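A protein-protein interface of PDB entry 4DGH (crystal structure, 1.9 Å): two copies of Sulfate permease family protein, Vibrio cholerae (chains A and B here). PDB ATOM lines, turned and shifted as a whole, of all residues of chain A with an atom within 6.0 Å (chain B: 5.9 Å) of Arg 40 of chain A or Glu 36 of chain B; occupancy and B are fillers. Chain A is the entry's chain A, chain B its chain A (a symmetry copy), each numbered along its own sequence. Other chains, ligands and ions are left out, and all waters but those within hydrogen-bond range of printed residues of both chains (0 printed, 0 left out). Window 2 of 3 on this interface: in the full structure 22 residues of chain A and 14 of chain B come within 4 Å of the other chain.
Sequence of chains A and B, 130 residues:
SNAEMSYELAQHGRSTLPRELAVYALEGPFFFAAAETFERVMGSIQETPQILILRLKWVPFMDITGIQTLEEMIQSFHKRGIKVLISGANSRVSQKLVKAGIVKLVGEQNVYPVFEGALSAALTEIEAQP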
ATOM      1  N   ALA A  33     -24.544 -16.630 -15.668  1.00  0.00           N
ATOM      2  CA  ALA A  33     -25.145 -15.560 -16.503  1.00  0.00           C
ATOM      3  C   ALA A  33     -24.047 -14.940 -17.415  1.00  0.00           C
ATOM      4  O   ALA A  33     -24.266 -14.731 -18.614  1.00  0.00           O
ATOM      5  CB  ALA A  33     -25.856 -14.476 -15.654  1.00  0.00           C
ATOM      6  N   ALA A  35     -21.181 -16.566 -18.354  1.00  0.00           N
ATOM      7  CA  ALA A  35     -20.854 -17.572 -19.336  1.00  0.00           C
ATOM      8  C   ALA A  35     -21.809 -17.394 -20.521  1.00  0.00           C
ATOM      9  O   ALA A  35     -21.383 -17.442 -21.650  1.00  0.00           O
ATOM     10  CB  ALA A  35     -21.029 -18.963 -18.726  1.00  0.00           C
ATOM     11  N   GLU A  36     -23.093 -17.188 -20.250  1.00  0.00           N
ATOM     12  CA  GLU A  36     -24.106 -17.180 -21.317  1.00  0.00           C
ATOM     13  C   GLU A  36     -23.896 -15.957 -22.240  1.00  0.00           C
ATOM     14  O   GLU A  36     -23.886 -16.067 -23.462  1.00  0.00           O
ATOM     15  CB  GLU A  36     -25.513 -17.108 -20.705  1.00  0.00           C
ATOM     16  CG  GLU A  36     -26.637 -17.454 -21.657  1.00  0.00           C
ATOM     17  CD  GLU A  36     -28.005 -17.190 -21.036  1.00  0.00           C
ATOM     18  OE1 GLU A  36     -28.177 -17.372 -19.795  1.00  0.00           O
ATOM     19  OE2 GLU A  36     -28.909 -16.778 -21.795  1.00  0.00           O
ATOM     20  N   THR A  37     -23.690 -14.812 -21.625  1.00  0.00           N
ATOM     21  CA  THR A  37     -23.429 -13.579 -22.360  1.00  0.00           C
ATOM     22  C   THR A  37     -22.168 -13.690 -23.223  1.00  0.00           C
ATOM     23  O   THR A  37     -22.171 -13.340 -24.418  1.00  0.00           O
ATOM     24  CB  THR A  37     -23.351 -12.429 -21.355  1.00  0.00           C
ATOM     25  OG1 THR A  37     -24.600 -12.414 -20.629  1.00  0.00           O
ATOM     26  CG2 THR A  37     -23.151 -11.092 -22.091  1.00  0.00           C
ATOM     27  N   PHE A  38     -21.115 -14.236 -22.641  1.00  0.00           N
ATOM     28  CA  PHE A  38     -19.860 -14.249 -23.336  1.00  0.00           C
ATOM     29  C   PHE A  38     -19.929 -15.196 -24.540  1.00  0.00           C
ATOM     30  O   PHE A  38     -19.402 -14.915 -25.611  1.00  0.00           O
ATOM     31  CB  PHE A  38     -18.722 -14.658 -22.445  1.00  0.00           C
ATOM     32  CG  PHE A  38     -17.424 -14.279 -23.025  1.00  0.00           C
ATOM     33  CD1 PHE A  38     -17.191 -12.966 -23.385  1.00  0.00           C
ATOM     34  CD2 PHE A  38     -16.473 -15.216 -23.337  1.00  0.00           C
ATOM     35  CE1 PHE A  38     -15.991 -12.574 -23.982  1.00  0.00           C
ATOM     36  CE2 PHE A  38     -15.248 -14.820 -23.888  1.00  0.00           C
ATOM     37  CZ  PHE A  38     -15.028 -13.495 -24.256  1.00  0.00           C
ATOM     38  N   GLU A  39     -20.613 -16.312 -24.330  1.00  0.00           N
ATOM     39  CA  GLU A  39     -20.861 -17.276 -25.351  1.00  0.00           C
ATOM     40  C   GLU A  39     -21.661 -16.598 -26.481  1.00  0.00           C
ATOM     41  O   GLU A  39     -21.342 -16.727 -27.658  1.00  0.00           O
ATOM     42  CB  GLU A  39     -21.646 -18.385 -24.639  1.00  0.00           C
ATOM     43  CG  GLU A  39     -21.735 -19.690 -25.386  1.00  0.00           C
ATOM     44  CD  GLU A  39     -22.382 -20.817 -24.548  1.00  0.00           C
ATOM     45  OE1 GLU A  39     -22.344 -20.758 -23.292  1.00  0.00           O
ATOM     46  OE2 GLU A  39     -22.936 -21.766 -25.175  1.00  0.00           O
ATOM     47  N   ARG A  40     -22.687 -15.818 -26.112  1.00  0.00           N
ATOM     48  CA  ARG A  40     -23.462 -15.056 -27.092  1.00  0.00           C
ATOM     49  C   ARG A  40     -22.626 -14.053 -27.855  1.00  0.00           C
ATOM     50  O   ARG A  40     -22.681 -14.009 -29.040  1.00  0.00           O
ATOM     51  CB  ARG A  40     -24.725 -14.457 -26.435  1.00  0.00           C
ATOM     52  CG  ARG A  40     -25.606 -13.574 -27.336  1.00  0.00           C
ATOM     53  CD  ARG A  40     -27.004 -13.279 -26.718  1.00  0.00           C
ATOM     54  NE  ARG A  40     -26.959 -12.768 -25.334  1.00  0.00           N
ATOM     55  CZ  ARG A  40     -27.285 -13.492 -24.248  1.00  0.00           C
ATOM     56  NH1 ARG A  40     -27.696 -14.771 -24.397  1.00  0.00           N
ATOM     57  NH2 ARG A  40     -27.184 -12.950 -23.019  1.00  0.00           N
ATOM     58  N   VAL A  41     -21.758 -13.323 -27.189  1.00  0.00           N
ATOM     59  CA  VAL A  41     -20.913 -12.337 -27.835  1.00  0.00           C
ATOM     60  C   VAL A  41     -19.970 -13.026 -28.832  1.00  0.00           C
ATOM     61  O   VAL A  41     -19.804 -12.573 -29.966  1.00  0.00           O
ATOM     62  CB  VAL A  41     -20.007 -11.657 -26.791  1.00  0.00           C
ATOM     63  CG1 VAL A  41     -18.948 -10.805 -27.505  1.00  0.00           C
ATOM     64  CG2 VAL A  41     -20.817 -10.777 -25.843  1.00  0.00           C
ATOM     65  N   MET A  42     -19.355 -14.109 -28.390  1.00  0.00           N
ATOM     66  CA  MET A  42     -18.351 -14.759 -29.235  1.00  0.00           C
ATOM     67  C   MET A  42     -19.029 -15.305 -30.488  1.00  0.00           C
ATOM     68  O   MET A  42     -18.413 -15.401 -31.562  1.00  0.00           O
ATOM     69  CB  MET A  42     -17.687 -15.890 -28.423  1.00  0.00           C
ATOM     70  CG  MET A  42     -16.440 -16.358 -29.147  1.00  0.00           C
ATOM     71  SD  MET A  42     -15.057 -14.940 -28.923  1.00  0.00           S
ATOM     72  CE  MET A  42     -13.989 -15.285 -27.311  1.00  0.00           C
ATOM     73  N   GLY A  43     -20.265 -15.731 -30.339  1.00  0.00           N
ATOM     74  CA  GLY A  43     -21.072 -16.215 -31.488  1.00  0.00           C
ATOM     75  C   GLY A  43     -21.506 -15.123 -32.444  1.00  0.00           C
ATOM     76  O   GLY A  43     -21.694 -15.379 -33.664  1.00  0.00           O
ATOM     77  N   SER A  44     -21.680 -13.908 -31.934  1.00  0.00           N
ATOM     78  CA  SER A  44     -22.282 -12.824 -32.763  1.00  0.00           C
ATOM     79  C   SER A  44     -21.275 -11.904 -33.429  1.00  0.00           C
ATOM     80  O   SER A  44     -21.534 -11.333 -34.511  1.00  0.00           O
ATOM     81  CB  SER A  44     -23.377 -12.038 -31.998  1.00  0.00           C
ATOM     82  OG  SER A  44     -22.802 -11.076 -31.129  1.00  0.00           O
ATOM     83  N   ILE A  45     -20.127 -11.739 -32.816  1.00  0.00           N
ATOM     84  CA  ILE A  45     -19.107 -10.896 -33.425  1.00  0.00           C
ATOM     85  C   ILE A  45     -18.546 -11.516 -34.703  1.00  0.00           C
ATOM     86  O   ILE A  45     -18.550 -12.741 -34.886  1.00  0.00           O
ATOM     87  CB  ILE A  45     -17.935 -10.575 -32.487  1.00  0.00           C
ATOM     88  CG1 ILE A  45     -17.235 -11.895 -32.096  1.00  0.00           C
ATOM     89  CG2 ILE A  45     -18.457  -9.708 -31.334  1.00  0.00           C
ATOM     90  CD1 ILE A  45     -15.988 -11.732 -31.220  1.00  0.00           C
ATOM     91  N   PHE B  31     -17.904  -5.814 -19.927  1.00  0.00           N
ATOM     92  CA  PHE B  31     -19.038  -4.903 -19.816  1.00  0.00           C
ATOM     93  C   PHE B  31     -20.112  -5.381 -20.790  1.00  0.00           C
ATOM     94  O   PHE B  31     -21.071  -4.714 -20.957  1.00  0.00           O
ATOM     95  CB  PHE B  31     -18.609  -3.474 -20.149  1.00  0.00           C
ATOM     96  CG  PHE B  31     -17.892  -3.373 -21.498  1.00  0.00           C
ATOM     97  CD1 PHE B  31     -18.634  -3.298 -22.685  1.00  0.00           C
ATOM     98  CD2 PHE B  31     -16.494  -3.402 -21.568  1.00  0.00           C
ATOM     99  CE1 PHE B  31     -18.005  -3.214 -23.926  1.00  0.00           C
ATOM    100  CE2 PHE B  31     -15.881  -3.331 -22.809  1.00  0.00           C
ATOM    101  CZ  PHE B  31     -16.632  -3.268 -23.981  1.00  0.00           C
ATOM    102  N   PHE B  32     -19.966  -6.582 -21.375  1.00  0.00           N
ATOM    103  CA  PHE B  32     -20.885  -7.060 -22.462  1.00  0.00           C
ATOM    104  C   PHE B  32     -22.358  -7.083 -22.059  1.00  0.00           C
ATOM    105  O   PHE B  32     -23.211  -6.640 -22.819  1.00  0.00           O
ATOM    106  CB  PHE B  32     -20.504  -8.481 -23.017  1.00  0.00           C
ATOM    107  CG  PHE B  32     -19.016  -8.706 -23.163  1.00  0.00           C
ATOM    108  CD1 PHE B  32     -18.303  -8.106 -24.204  1.00  0.00           C
ATOM    109  CD2 PHE B  32     -18.320  -9.465 -22.225  1.00  0.00           C
ATOM    110  CE1 PHE B  32     -16.915  -8.261 -24.314  1.00  0.00           C
ATOM    111  CE2 PHE B  32     -16.934  -9.624 -22.334  1.00  0.00           C
ATOM    112  CZ  PHE B  32     -16.227  -9.018 -23.355  1.00  0.00           C
ATOM    113  N   ALA B  33     -22.670  -7.607 -20.890  1.00  0.00           N
ATOM    114  CA  ALA B  33     -24.109  -7.749 -20.549  1.00  0.00           C
ATOM    115  C   ALA B  33     -24.742  -6.337 -20.384  1.00  0.00           C
ATOM    116  O   ALA B  33     -25.833  -6.070 -20.899  1.00  0.00           O
ATOM    117  CB  ALA B  33     -24.334  -8.623 -19.289  1.00  0.00           C
ATOM    118  N   ALA B  34     -24.007  -5.437 -19.730  1.00  0.00           N
ATOM    119  CA  ALA B  34     -24.381  -4.008 -19.645  1.00  0.00           C
ATOM    120  C   ALA B  34     -24.466  -3.278 -20.965  1.00  0.00           C
ATOM    121  O   ALA B  34     -25.379  -2.506 -21.194  1.00  0.00           O
ATOM    122  CB  ALA B  34     -23.388  -3.285 -18.768  1.00  0.00           C
ATOM    123  N   ALA B  35     -23.505  -3.492 -21.837  1.00  0.00           N
ATOM    124  CA  ALA B  35     -23.561  -2.914 -23.160  1.00  0.00           C
ATOM    125  C   ALA B  35     -24.890  -3.334 -23.795  1.00  0.00           C
ATOM    126  O   ALA B  35     -25.554  -2.524 -24.394  1.00  0.00           O
ATOM    127  CB  ALA B  35     -22.391  -3.433 -23.997  1.00  0.00           C
ATOM    128  N   GLU B  36     -25.263  -4.602 -23.657  1.00  0.00           N
ATOM    129  CA  GLU B  36     -26.430  -5.135 -24.377  1.00  0.00           C
ATOM    130  C   GLU B  36     -27.728  -4.483 -23.845  1.00  0.00           C
ATOM    131  O   GLU B  36     -28.577  -4.025 -24.604  1.00  0.00           O
ATOM    132  CB  GLU B  36     -26.519  -6.656 -24.180  1.00  0.00           C
ATOM    133  CG  GLU B  36     -27.443  -7.368 -25.144  1.00  0.00           C
ATOM    134  CD  GLU B  36     -27.617  -8.839 -24.778  1.00  0.00           C
ATOM    135  OE1 GLU B  36     -26.650  -9.480 -24.273  1.00  0.00           O
ATOM    136  OE2 GLU B  36     -28.739  -9.350 -24.981  1.00  0.00           O
ATOM    137  N   THR B  37     -27.833  -4.417 -22.535  1.00  0.00           N
ATOM    138  CA  THR B  37     -28.976  -3.788 -21.884  1.00  0.00           C
ATOM    139  C   THR B  37     -29.106  -2.311 -22.272  1.00  0.00           C
ATOM    140  O   THR B  37     -30.197  -1.834 -22.639  1.00  0.00           O
ATOM    141  CB  THR B  37     -28.839  -3.986 -20.375  1.00  0.00           C
ATOM    142  OG1 THR B  37     -28.753  -5.409 -20.139  1.00  0.00           O
ATOM    143  CG2 THR B  37     -30.063  -3.403 -19.647  1.00  0.00           C
ATOM    144  N   PHE B  38     -27.988  -1.608 -22.256  1.00  0.00           N
ATOM    145  CA  PHE B  38     -28.049  -0.191 -22.472  1.00  0.00           C
ATOM    146  C   PHE B  38     -28.446   0.109 -23.922  1.00  0.00           C
ATOM    147  O   PHE B  38     -29.213   1.023 -24.203  1.00  0.00           O
ATOM    148  CB  PHE B  38     -26.745   0.487 -22.161  1.00  0.00           C
ATOM    149  CG  PHE B  38     -26.923   1.936 -21.985  1.00  0.00           C
ATOM    150  CD1 PHE B  38     -27.842   2.407 -21.067  1.00  0.00           C
ATOM    151  CD2 PHE B  38     -26.291   2.845 -22.795  1.00  0.00           C
ATOM    152  CE1 PHE B  38     -28.075   3.774 -20.902  1.00  0.00           C
ATOM    153  CE2 PHE B  38     -26.484   4.217 -22.599  1.00  0.00           C
ATOM    154  CZ  PHE B  38     -27.420   4.680 -21.677  1.00  0.00           C
ATOM    155  N   GLU B  39     -27.912  -0.704 -24.823  1.00  0.00           N
ATOM    156  CA  GLU B  39     -28.226  -0.639 -26.212  1.00  0.00           C
ATOM    157  C   GLU B  39     -29.738  -0.891 -26.385  1.00  0.00           C
ATOM    158  O   GLU B  39     -30.431  -0.168 -27.091  1.00  0.00           O
ATOM    159  CB  GLU B  39     -27.357  -1.732 -26.846  1.00  0.00           C
ATOM    160  CG  GLU B  39     -27.220  -1.655 -28.345  1.00  0.00           C
ATOM    161  CD  GLU B  39     -26.197  -2.669 -28.905  1.00  0.00           C
ATOM    162  OE1 GLU B  39     -25.278  -3.100 -28.163  1.00  0.00           O
ATOM    163  OE2 GLU B  39     -26.335  -3.033 -30.110  1.00  0.00           O
ATOM    164  N   ARG B  40     -30.266  -1.904 -25.683  1.00  0.00           N
ATOM    165  CA  ARG B  40     -31.703  -2.180 -25.701  1.00  0.00           C
ATOM    166  C   ARG B  40     -32.532  -1.031 -25.174  1.00  0.00           C
ATOM    167  O   ARG B  40     -33.463  -0.633 -25.795  1.00  0.00           O
ATOM    168  CB  ARG B  40     -32.000  -3.537 -25.023  1.00  0.00           C
ATOM    169  CG  ARG B  40     -33.484  -3.931 -24.912  1.00  0.00           C
ATOM    170  CD  ARG B  40     -33.688  -5.424 -24.526  1.00  0.00           C
ATOM    171  NE  ARG B  40     -32.923  -5.855 -23.340  1.00  0.00           N
ATOM    172  CZ  ARG B  40     -31.824  -6.629 -23.387  1.00  0.00           C
ATOM    173  NH1 ARG B  40     -31.370  -7.070 -24.581  1.00  0.00           N
ATOM    174  NH2 ARG B  40     -31.171  -6.947 -22.253  1.00  0.00           N
ATOM    175  N   VAL B  41     -32.129  -0.412 -24.086  1.00  0.00           N
ATOM    176  CA  VAL B  41     -32.859   0.700 -23.508  1.00  0.00           C
ATOM    177  C   VAL B  41     -32.881   1.880 -24.490  1.00  0.00           C
ATOM    178  O   VAL B  41     -33.922   2.500 -24.715  1.00  0.00           O
ATOM    179  CB  VAL B  41     -32.132   1.207 -22.248  1.00  0.00           C
ATOM    180  CG1 VAL B  41     -32.760   2.531 -21.788  1.00  0.00           C
ATOM    181  CG2 VAL B  41     -32.206   0.186 -21.117  1.00  0.00           C
ATOM    182  N   THR B  69     -17.896  -5.180 -29.494  1.00  0.00           N
ATOM    183  CA  THR B  69     -19.078  -4.821 -28.695  1.00  0.00           C
ATOM    184  C   THR B  69     -19.239  -3.323 -28.571  1.00  0.00           C
ATOM    185  O   THR B  69     -20.357  -2.792 -28.718  1.00  0.00           O
ATOM    186  CB  THR B  69     -18.972  -5.535 -27.332  1.00  0.00           C
ATOM    187  OG1 THR B  69     -18.908  -6.926 -27.603  1.00  0.00           O
ATOM    188  CG2 THR B  69     -20.202  -5.323 -26.454  1.00  0.00           C
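The side-chain carboxylate (OE1) of Glu 36 of chain B lies within salt-bridge range of the guanidinium group (NE) of Arg 40 of chain A (3.5 Å).
OG1 of Thr 37 of chain A is in hydrogen-bond range of O of Ala 33 of chain A (3.1 Å). The side-chain carboxylate of Glu 36 of chain A is in salt-bridge range of the guanidinium group of Arg 40 of chain A (3.5 Å). OG1 of Thr 37 of chain B sits at hydrogen-bond distance from O of Ala 33 of chain B. OE2 of Glu 36 of chain B lies within salt-bridge range of NH1 of Arg 40 of chain B, at 3.5 Å.
Phe 32 of chain B touches Thr 37 of chain A. Thr 37 of chain A touches Ala 33 of chain B (CG2 to N, 3.7 Å). CE1 of Phe 38 of chain A touches CE2 of Phe 32 of chain B, 3.5 Å away. CG2 of Val 41 of chain A touches CB of Phe 32 of chain B, at 3.7 Å. CG1 of Val 41 of chain A touches OG1 of Thr 69 of chain B, 3.9 Å away.
Of the printed residues of chain B, Arg 40 of chain A touches Glu 36. Glu 36 of chain B touches one residue of chain A. Printed residues of chain B within 4 Å of Val 41 of chain A: Phe 32 and Thr 69. Of the printed residues of chain A, Ala 33 of chain B touches Thr 37. Of the printed residues of chain B, Thr 37 of chain A touches Phe 32 and Ala 33. Phe 31 of chain B touches none of the printed residues of chain A. The nearest residue of chain A that does not touch Glu 36 of chain B is Thr 37 of chain A (4.4 Å). The nearest printed residue of chain A that does not touch Phe 32 of chain B is Ile 45 of chain A (7.3 Å).
Of the 12 printed residues of chain A, 4 touch a printed residue of chain B. Along chain A the printed residues that touch a printed residue of chain B span positions 37 to 41. Among the printed residues, 6 pairs touch across the chains.
Thr 37 of chain A touches Ala 33 of chain B, but with the chains exchanged Ala 33 of chain A does not touch Thr 37 of chain B (10.5 Å). Arg 40 of chain A touches Glu 36 of chain B, but with the chains exchanged Glu 36 of chain A does not touch Arg 40 of chain B (10.1 Å). Positions printed for both chains: 33, 35, 36, 37, 38, 39, 40 and 41. Of the 6 pairs that touch across the chains among the printed residues, none has its exchanged pair printed and touching as well.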
